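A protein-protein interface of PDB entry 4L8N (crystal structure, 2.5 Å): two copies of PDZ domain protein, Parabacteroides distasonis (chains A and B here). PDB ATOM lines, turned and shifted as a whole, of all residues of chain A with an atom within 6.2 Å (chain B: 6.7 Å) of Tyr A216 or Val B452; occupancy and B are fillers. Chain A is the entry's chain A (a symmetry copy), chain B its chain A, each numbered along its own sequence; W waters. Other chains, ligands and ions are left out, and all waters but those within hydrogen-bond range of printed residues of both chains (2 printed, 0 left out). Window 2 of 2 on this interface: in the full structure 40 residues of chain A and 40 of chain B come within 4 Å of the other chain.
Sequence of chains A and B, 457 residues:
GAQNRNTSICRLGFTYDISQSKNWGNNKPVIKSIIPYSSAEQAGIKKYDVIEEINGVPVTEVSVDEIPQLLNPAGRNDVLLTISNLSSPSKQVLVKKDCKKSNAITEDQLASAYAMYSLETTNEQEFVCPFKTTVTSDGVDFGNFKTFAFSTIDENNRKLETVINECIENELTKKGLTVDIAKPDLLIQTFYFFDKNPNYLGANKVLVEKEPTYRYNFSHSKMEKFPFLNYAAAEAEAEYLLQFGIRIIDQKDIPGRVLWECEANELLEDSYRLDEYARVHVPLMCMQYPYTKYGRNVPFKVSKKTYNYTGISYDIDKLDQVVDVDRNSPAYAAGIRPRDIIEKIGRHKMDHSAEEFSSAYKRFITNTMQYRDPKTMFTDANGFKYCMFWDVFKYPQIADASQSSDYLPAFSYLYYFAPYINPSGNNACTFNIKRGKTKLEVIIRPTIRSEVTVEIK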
ATOM      1  N   TYR A 214      12.263   8.777   3.333  1.00  0.00           N
ATOM      2  CA  TYR A 214      12.947   8.889   4.625  1.00  0.00           C
ATOM      3  C   TYR A 214      14.042   9.921   4.498  1.00  0.00           C
ATOM      4  O   TYR A 214      14.738   9.969   3.478  1.00  0.00           O
ATOM      5  CB  TYR A 214      13.494   7.559   5.150  1.00  0.00           C
ATOM      6  CG  TYR A 214      12.415   6.538   5.429  1.00  0.00           C
ATOM      7  CD1 TYR A 214      11.647   6.600   6.590  1.00  0.00           C
ATOM      8  CD2 TYR A 214      12.145   5.515   4.524  1.00  0.00           C
ATOM      9  CE1 TYR A 214      10.631   5.672   6.837  1.00  0.00           C
ATOM     10  CE2 TYR A 214      11.157   4.563   4.779  1.00  0.00           C
ATOM     11  CZ  TYR A 214      10.383   4.660   5.922  1.00  0.00           C
ATOM     12  OH  TYR A 214       9.392   3.729   6.149  1.00  0.00           O
ATOM     13  N   ARG A 215      14.106  10.837   5.460  1.00  0.00           N
ATOM     14  CA  ARG A 215      15.133  11.873   5.487  1.00  0.00           C
ATOM     15  C   ARG A 215      15.609  12.035   6.909  1.00  0.00           C
ATOM     16  O   ARG A 215      14.887  11.668   7.843  1.00  0.00           O
ATOM     17  CB  ARG A 215      14.637  13.211   4.915  1.00  0.00           C
ATOM     18  CG  ARG A 215      14.039  13.077   3.542  1.00  0.00           C
ATOM     19  CD  ARG A 215      14.479  14.128   2.585  1.00  0.00           C
ATOM     20  NE  ARG A 215      13.981  13.755   1.270  1.00  0.00           N
ATOM     21  CZ  ARG A 215      13.320  14.570   0.478  1.00  0.00           C
ATOM     22  NH1 ARG A 215      13.115  15.826   0.833  1.00  0.00           N
ATOM     23  NH2 ARG A 215      12.862  14.142  -0.688  1.00  0.00           N
ATOM     24  N   TYR A 216      16.808  12.604   7.085  1.00  0.00           N
ATOM     25  CA  TYR A 216      17.312  12.809   8.422  1.00  0.00           C
ATOM     26  C   TYR A 216      16.898  14.206   8.902  1.00  0.00           C
ATOM     27  O   TYR A 216      17.004  15.192   8.166  1.00  0.00           O
ATOM     28  CB  TYR A 216      18.819  12.599   8.483  1.00  0.00           C
ATOM     29  CG  TYR A 216      19.334  12.563   9.900  1.00  0.00           C
ATOM     30  CD1 TYR A 216      19.222  11.418  10.669  1.00  0.00           C
ATOM     31  CD2 TYR A 216      19.954  13.674  10.469  1.00  0.00           C
ATOM     32  CE1 TYR A 216      19.697  11.376  11.976  1.00  0.00           C
ATOM     33  CE2 TYR A 216      20.411  13.652  11.786  1.00  0.00           C
ATOM     34  CZ  TYR A 216      20.304  12.492  12.528  1.00  0.00           C
ATOM     35  OH  TYR A 216      20.813  12.426  13.807  1.00  0.00           O
ATOM     36  N   ASN A 217      16.399  14.268  10.128  1.00  0.00           N
ATOM     37  CA  ASN A 217      15.927  15.501  10.716  1.00  0.00           C
ATOM     38  C   ASN A 217      16.856  15.858  11.886  1.00  0.00           C
ATOM     39  O   ASN A 217      16.755  15.251  12.963  1.00  0.00           O
ATOM     40  CB  ASN A 217      14.454  15.320  11.147  1.00  0.00           C
ATOM     41  CG  ASN A 217      13.769  16.521  11.750  1.00  0.00           C
ATOM     42  OD1 ASN A 217      12.634  16.422  12.209  1.00  0.00           O
ATOM     43  ND2 ASN A 217      14.420  17.676  11.785  1.00  0.00           N
ATOM     44  N   PHE A 218      17.771  16.842  11.658  1.00  0.00           N
ATOM     45  CA  PHE A 218      18.784  17.274  12.639  1.00  0.00           C
ATOM     46  C   PHE A 218      18.142  17.821  13.911  1.00  0.00           C
ATOM     47  O   PHE A 218      18.654  17.539  15.004  1.00  0.00           O
ATOM     48  CB  PHE A 218      19.768  18.290  12.046  1.00  0.00           C
ATOM     49  CG  PHE A 218      20.886  17.727  11.181  1.00  0.00           C
ATOM     50  CD1 PHE A 218      22.053  17.216  11.759  1.00  0.00           C
ATOM     51  CD2 PHE A 218      20.796  17.746   9.790  1.00  0.00           C
ATOM     52  CE1 PHE A 218      23.102  16.728  10.955  1.00  0.00           C
ATOM     53  CE2 PHE A 218      21.844  17.252   8.988  1.00  0.00           C
ATOM     54  CZ  PHE A 218      22.996  16.753   9.577  1.00  0.00           C
ATOM     55  N   HIS A 220      15.532  16.768  15.419  1.00  0.00           N
ATOM     56  CA  HIS A 220      15.113  15.649  16.275  1.00  0.00           C
ATOM     57  C   HIS A 220      16.171  14.552  16.368  1.00  0.00           C
ATOM     58  O   HIS A 220      15.987  13.602  17.138  1.00  0.00           O
ATOM     59  CB  HIS A 220      13.774  15.061  15.793  1.00  0.00           C
ATOM     60  CG  HIS A 220      12.645  16.024  15.951  1.00  0.00           C
ATOM     61  ND1 HIS A 220      11.780  16.298  14.905  1.00  0.00           N
ATOM     62  CD2 HIS A 220      12.322  16.811  17.010  1.00  0.00           C
ATOM     63  CE1 HIS A 220      10.950  17.222  15.364  1.00  0.00           C
ATOM     64  NE2 HIS A 220      11.235  17.558  16.631  1.00  0.00           N
ATOM     65  N   SER A 221      17.282  14.688  15.589  1.00  0.00           N
ATOM     66  CA  SER A 221      18.423  13.753  15.557  1.00  0.00           C
ATOM     67  C   SER A 221      17.972  12.298  15.257  1.00  0.00           C
ATOM     68  O   SER A 221      18.363  11.349  15.952  1.00  0.00           O
ATOM     69  CB  SER A 221      19.241  13.839  16.851  1.00  0.00           C
ATOM     70  OG  SER A 221      20.109  14.961  16.783  1.00  0.00           O
ATOM     71  N   LYS A 222      17.139  12.148  14.206  1.00  0.00           N
ATOM     72  CA  LYS A 222      16.609  10.864  13.770  1.00  0.00           C
ATOM     73  C   LYS A 222      16.091  10.907  12.339  1.00  0.00           C
ATOM     74  O   LYS A 222      15.765  11.986  11.816  1.00  0.00           O
ATOM     75  CB  LYS A 222      15.495  10.358  14.724  1.00  0.00           C
ATOM     76  CG  LYS A 222      14.226  11.206  14.791  1.00  0.00           C
ATOM     77  CD  LYS A 222      13.158  10.540  15.642  1.00  0.00           C
ATOM     78  CE  LYS A 222      11.914  11.389  15.732  1.00  0.00           C
ATOM     79  NZ  LYS A 222      11.176  11.160  17.002  1.00  0.00           N
ATOM     80  N   MET A 223      16.029   9.717  11.696  1.00  0.00           N
ATOM     81  CA  MET A 223      15.419   9.540  10.366  1.00  0.00           C
ATOM     82  C   MET A 223      13.905   9.641  10.544  1.00  0.00           C
ATOM     83  O   MET A 223      13.384   9.211  11.575  1.00  0.00           O
ATOM     84  CB  MET A 223      15.772   8.163   9.740  1.00  0.00           C
ATOM     85  CG  MET A 223      17.217   8.005   9.311  1.00  0.00           C
ATOM     86  SD  MET A 223      17.631   8.985   7.748  1.00  0.00           S
ATOM     87  CE  MET A 223      16.819   8.029   6.460  1.00  0.00           C
ATOM     88  N   GLU A 224      13.200  10.203   9.570  1.00  0.00           N
ATOM     89  CA  GLU A 224      11.748  10.346   9.663  1.00  0.00           C
ATOM     90  C   GLU A 224      11.109  10.097   8.331  1.00  0.00           C
ATOM     91  O   GLU A 224      11.753  10.288   7.295  1.00  0.00           O
ATOM     92  CB  GLU A 224      11.364  11.763  10.144  1.00  0.00           C
ATOM     93  CG  GLU A 224      11.603  12.036  11.617  1.00  0.00           C
ATOM     94  CD  GLU A 224      11.328  13.452  12.097  1.00  0.00           C
ATOM     95  OE1 GLU A 224      10.811  14.268  11.299  1.00  0.00           O
ATOM     96  OE2 GLU A 224      11.597  13.731  13.290  1.00  0.00           O
ATOM     97  N   PHE A 226       8.535  11.225   5.514  1.00  0.00           N
ATOM     98  CA  PHE A 226       8.084  12.527   5.051  1.00  0.00           C
ATOM     99  C   PHE A 226       6.995  12.319   4.025  1.00  0.00           C
ATOM    100  O   PHE A 226       7.067  11.341   3.276  1.00  0.00           O
ATOM    101  CB  PHE A 226       9.259  13.381   4.504  1.00  0.00           C
ATOM    102  CG  PHE A 226      10.069  14.024   5.613  1.00  0.00           C
ATOM    103  CD1 PHE A 226      11.098  13.330   6.238  1.00  0.00           C
ATOM    104  CD2 PHE A 226       9.767  15.303   6.065  1.00  0.00           C
ATOM    105  CE1 PHE A 226      11.811  13.904   7.289  1.00  0.00           C
ATOM    106  CE2 PHE A 226      10.482  15.875   7.123  1.00  0.00           C
ATOM    107  CZ  PHE A 226      11.489  15.167   7.732  1.00  0.00           C
ATOM    108  N   PRO B  36      34.519   9.822  14.663  1.00  0.00           N
ATOM    109  CA  PRO B  36      34.328  10.196  16.070  1.00  0.00           C
ATOM    110  C   PRO B  36      35.297   9.494  16.980  1.00  0.00           C
ATOM    111  O   PRO B  36      35.692   8.364  16.703  1.00  0.00           O
ATOM    112  CB  PRO B  36      32.898   9.743  16.374  1.00  0.00           C
ATOM    113  CG  PRO B  36      32.220   9.663  15.019  1.00  0.00           C
ATOM    114  CD  PRO B  36      33.295   9.216  14.093  1.00  0.00           C
ATOM    115  N   PHE B 127      19.580   7.952   1.895  1.00  0.00           N
ATOM    116  CA  PHE B 127      18.461   8.687   1.309  1.00  0.00           C
ATOM    117  C   PHE B 127      18.985   9.676   0.251  1.00  0.00           C
ATOM    118  O   PHE B 127      20.163  10.052   0.271  1.00  0.00           O
ATOM    119  CB  PHE B 127      17.620   9.387   2.364  1.00  0.00           C
ATOM    120  CG  PHE B 127      18.316  10.429   3.199  1.00  0.00           C
ATOM    121  CD1 PHE B 127      18.999  10.072   4.360  1.00  0.00           C
ATOM    122  CD2 PHE B 127      18.187  11.782   2.897  1.00  0.00           C
ATOM    123  CE1 PHE B 127      19.603  11.047   5.160  1.00  0.00           C
ATOM    124  CE2 PHE B 127      18.784  12.756   3.705  1.00  0.00           C
ATOM    125  CZ  PHE B 127      19.489  12.382   4.829  1.00  0.00           C
ATOM    126  N   VAL B 280      14.372  21.421   8.280  1.00  0.00           N
ATOM    127  CA  VAL B 280      14.897  20.082   8.001  1.00  0.00           C
ATOM    128  C   VAL B 280      15.964  20.111   6.901  1.00  0.00           C
ATOM    129  O   VAL B 280      17.023  19.522   7.076  1.00  0.00           O
ATOM    130  CB  VAL B 280      13.746  19.087   7.646  1.00  0.00           C
ATOM    131  CG1 VAL B 280      14.261  17.705   7.247  1.00  0.00           C
ATOM    132  CG2 VAL B 280      12.759  18.959   8.792  1.00  0.00           C
ATOM    133  N   HIS B 281      15.686  20.780   5.777  1.00  0.00           N
ATOM    134  CA  HIS B 281      16.506  20.743   4.559  1.00  0.00           C
ATOM    135  C   HIS B 281      17.584  21.800   4.428  1.00  0.00           C
ATOM    136  O   HIS B 281      18.597  21.474   3.806  1.00  0.00           O
ATOM    137  CB  HIS B 281      15.605  20.734   3.340  1.00  0.00           C
ATOM    138  CG  HIS B 281      14.725  19.523   3.334  1.00  0.00           C
ATOM    139  ND1 HIS B 281      13.499  19.520   3.983  1.00  0.00           N
ATOM    140  CD2 HIS B 281      14.950  18.287   2.816  1.00  0.00           C
ATOM    141  CE1 HIS B 281      12.994  18.302   3.798  1.00  0.00           C
ATOM    142  NE2 HIS B 281      13.822  17.528   3.092  1.00  0.00           N
ATOM    143  N   LEU B 284      20.804  20.092   5.234  1.00  0.00           N
ATOM    144  CA  LEU B 284      21.173  19.096   4.215  1.00  0.00           C
ATOM    145  C   LEU B 284      21.649  19.794   2.919  1.00  0.00           C
ATOM    146  O   LEU B 284      22.677  19.413   2.359  1.00  0.00           O
ATOM    147  CB  LEU B 284      20.007  18.135   3.906  1.00  0.00           C
ATOM    148  CG  LEU B 284      19.475  17.269   5.036  1.00  0.00           C
ATOM    149  CD1 LEU B 284      18.156  16.645   4.630  1.00  0.00           C
ATOM    150  CD2 LEU B 284      20.495  16.188   5.469  1.00  0.00           C
ATOM    151  N   VAL B 302      23.487   8.153   6.698  1.00  0.00           N
ATOM    152  CA  VAL B 302      23.393   8.361   8.152  1.00  0.00           C
ATOM    153  C   VAL B 302      23.830   7.072   8.863  1.00  0.00           C
ATOM    154  O   VAL B 302      23.209   6.030   8.681  1.00  0.00           O
ATOM    155  CB  VAL B 302      21.998   8.811   8.657  1.00  0.00           C
ATOM    156  CG1 VAL B 302      22.069   9.222  10.123  1.00  0.00           C
ATOM    157  CG2 VAL B 302      21.439   9.943   7.823  1.00  0.00           C
ATOM    158  N   SER B 303      24.899   7.154   9.641  1.00  0.00           N
ATOM    159  CA  SER B 303      25.459   6.048  10.418  1.00  0.00           C
ATOM    160  C   SER B 303      25.374   6.396  11.879  1.00  0.00           C
ATOM    161  O   SER B 303      26.071   7.316  12.330  1.00  0.00           O
ATOM    162  CB  SER B 303      26.909   5.775  10.025  1.00  0.00           C
ATOM    163  OG  SER B 303      27.022   5.445   8.650  1.00  0.00           O
ATOM    164  N   LYS B 304      24.486   5.709  12.623  1.00  0.00           N
ATOM    165  CA  LYS B 304      24.398   5.989  14.042  1.00  0.00           C
ATOM    166  C   LYS B 304      24.882   4.770  14.818  1.00  0.00           C
ATOM    167  O   LYS B 304      24.819   3.657  14.299  1.00  0.00           O
ATOM    168  CB  LYS B 304      22.999   6.478  14.456  1.00  0.00           C
ATOM    169  CG  LYS B 304      21.868   5.471  14.489  1.00  0.00           C
ATOM    170  CD  LYS B 304      20.686   6.138  15.168  1.00  0.00           C
ATOM    171  CE  LYS B 304      19.470   5.266  15.246  1.00  0.00           C
ATOM    172  NZ  LYS B 304      18.420   5.873  16.110  1.00  0.00           N
ATOM    173  N   LYS B 305      25.462   4.992  16.008  1.00  0.00           N
ATOM    174  CA  LYS B 305      25.981   3.916  16.871  1.00  0.00           C
ATOM    175  C   LYS B 305      26.093   4.365  18.324  1.00  0.00           C
ATOM    176  O   LYS B 305      26.631   5.435  18.609  1.00  0.00           O
ATOM    177  CB  LYS B 305      27.357   3.415  16.392  1.00  0.00           C
ATOM    178  CG  LYS B 305      27.916   2.225  17.191  1.00  0.00           C
ATOM    179  CD  LYS B 305      29.343   1.806  16.778  1.00  0.00           C
ATOM    180  CE  LYS B 305      29.373   1.291  15.356  1.00  0.00           C
ATOM    181  NZ  LYS B 305      30.657   0.649  15.019  1.00  0.00           N
ATOM    182  N   SER B 450      28.332   7.477  21.953  1.00  0.00           N
ATOM    183  CA  SER B 450      27.247   7.795  21.036  1.00  0.00           C
ATOM    184  C   SER B 450      27.814   8.597  19.896  1.00  0.00           C
ATOM    185  O   SER B 450      28.715   9.429  20.107  1.00  0.00           O
ATOM    186  CB  SER B 450      26.148   8.558  21.753  1.00  0.00           C
ATOM    187  OG  SER B 450      24.909   7.932  21.488  1.00  0.00           O
ATOM    188  N   GLU B 451      27.364   8.290  18.681  1.00  0.00           N
ATOM    189  CA  GLU B 451      27.846   8.937  17.466  1.00  0.00           C
ATOM    190  C   GLU B 451      26.834   8.829  16.330  1.00  0.00           C
ATOM    191  O   GLU B 451      26.151   7.818  16.178  1.00  0.00           O
ATOM    192  CB  GLU B 451      29.232   8.375  17.008  1.00  0.00           C
ATOM    193  CG  GLU B 451      29.402   6.857  17.072  1.00  0.00           C
ATOM    194  CD  GLU B 451      30.684   6.265  16.501  1.00  0.00           C
ATOM    195  OE1 GLU B 451      30.746   6.059  15.266  1.00  0.00           O
ATOM    196  OE2 GLU B 451      31.589   5.920  17.299  1.00  0.00           O
ATOM    197  N   VAL B 452      26.715   9.920  15.572  1.00  0.00           N
ATOM    198  CA  VAL B 452      25.933  10.056  14.339  1.00  0.00           C
ATOM    199  C   VAL B 452      26.838  10.720  13.301  1.00  0.00           C
ATOM    200  O   VAL B 452      27.389  11.785  13.576  1.00  0.00           O
ATOM    201  CB  VAL B 452      24.595  10.825  14.457  1.00  0.00           C
ATOM    202  CG1 VAL B 452      23.831  10.764  13.143  1.00  0.00           C
ATOM    203  CG2 VAL B 452      23.733  10.294  15.582  1.00  0.00           C
ATOM    204  N   THR B 453      26.991  10.095  12.136  1.00  0.00           N
ATOM    205  CA  THR B 453      27.716  10.628  10.995  1.00  0.00           C
ATOM    206  C   THR B 453      26.703  10.832   9.879  1.00  0.00           C
ATOM    207  O   THR B 453      26.004   9.894   9.499  1.00  0.00           O
ATOM    208  CB  THR B 453      28.868   9.699  10.613  1.00  0.00           C
ATOM    209  OG1 THR B 453      29.847   9.762  11.646  1.00  0.00           O
ATOM    210  CG2 THR B 453      29.499  10.057   9.268  1.00  0.00           C
ATOM    211  N   VAL B 454      26.567  12.074   9.412  1.00  0.00           N
ATOM    212  CA  VAL B 454      25.692  12.421   8.275  1.00  0.00           C
ATOM    213  C   VAL B 454      26.654  12.866   7.202  1.00  0.00           C
ATOM    214  O   VAL B 454      27.334  13.891   7.363  1.00  0.00           O
ATOM    215  CB  VAL B 454      24.579  13.436   8.586  1.00  0.00           C
ATOM    216  CG1 VAL B 454      23.681  13.654   7.361  1.00  0.00           C
ATOM    217  CG2 VAL B 454      23.748  12.973   9.783  1.00  0.00           C
HETATM  218  O   HOH W   1      17.482   7.743  13.529  1.00  0.00           O
HETATM  219  O   HOH W   2      17.709  17.699   9.010  1.00  0.00           O
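NE2 of His B281 is in hydrogen-bond range of NH1 of Arg A215, 2.9 Å away.
The backbone NH (N) of Tyr A216 is in hydrogen-bond range of the side-chain sulfur (SD) of Met A223 (3.8 Å).
The backbone carbonyl oxygen (O) of Arg A215 sits at hydrogen-bond distance from the backbone NH (N) of Glu A224 (2.8 Å).
OG of Ser A221 sits at hydrogen-bond distance from O of Phe A218 (3.5 Å).
The side-chain carboxylate (OE1) of Glu A224 lies close to the side-chain amide oxygen (OD1) of Asn A217.
OD1 of Asn A217 lies within hydrogen-bond range of ND1 of His A220, 2.8 Å away.
N of Asn A217 lies within hydrogen-bond range of O of Lys A222, 2.9 Å away.
Tyr A214 touches Phe B127.
N of Tyr A216 touches CZ of Phe B127, at 3.5 Å.
Tyr A216 touches Val B280 (O to CG1, 3.8 Å).
Val B302 touches Tyr A216.
Val B454 touches Tyr A216.
Asn A217 touches Val B280 (ND2 to CG2, 3.7 Å).
Phe A218 touches Val B454.
CD1 of Phe B127 touches CE of Met A223, at 3.7 Å.
Met A223 touches Val B302.
Phe A226 touches Val B280 (CZ to CG1, 3.8 Å).
Of the printed residues of chain B, Tyr A216 touches Phe B127, Val B280, Leu B284, Val B302, Val B452 and Val B454.
His A220 touches none of the printed residues of chain B.
Printed residues of chain B within 4 Å of Met A223: Phe B127 and Val B302.
Of the printed residues of chain A, Phe B127 touches Tyr A214, Tyr A216 and Met A223.
Of the printed residues of chain A, Leu B284 touches Tyr A216 (3.99 Å) and Phe A218 (3.9 Å).
Of the printed residues of chain A, Val B302 touches Tyr A216 (3.6 Å) and Met A223 (3.9 Å).
Ser B450 touches none of the printed residues of chain A.
Of chain A, only Tyr A216 (3.5 Å) comes within 4 Å of Val B452.
The nearest printed residue of chain B that does not touch Tyr A216 is Lys B304 (6.2 Å).
The nearest printed residue of chain A that does not touch Val B302 is Arg A215 (6.3 Å).
Hydrophobic or aromatic side chains of chain B that line the printed part of chain A: Phe B127, Val B280, His B281, Leu B284, Val B302, Val B452 and Val B454.
Of the 11 printed residues of chain A, 7 touch a printed residue of chain B.
Printed residues of chain A that touch a printed residue of chain B: Tyr A214, Arg A215, Tyr A216, Asn A217, Phe A218, Met A223 and Phe A226.
Hydrophobic or aromatic side chains of chain A that line the printed part of chain B: Tyr A216, Phe A218, Met A223 and Phe A226.
Among the printed residues, 14 pairs touch across the chains.
Among the printed residues, no Asp or Glu carboxylate lies within 4 Å of a Lys or Arg side-chain nitrogen of the other chain.
No position is printed for both chains.
Of the 14 pairs that touch across the chains among the printed residues, none has its exchanged pair printed and touching as well.
Water W2 lies within hydrogen-bond range of O of Tyr A216, O of Val B280 and N of Phe A218.
Water W1 bridges N of Met A223 (3.1 Å) and NZ of Lys B304 (3.3 Å).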
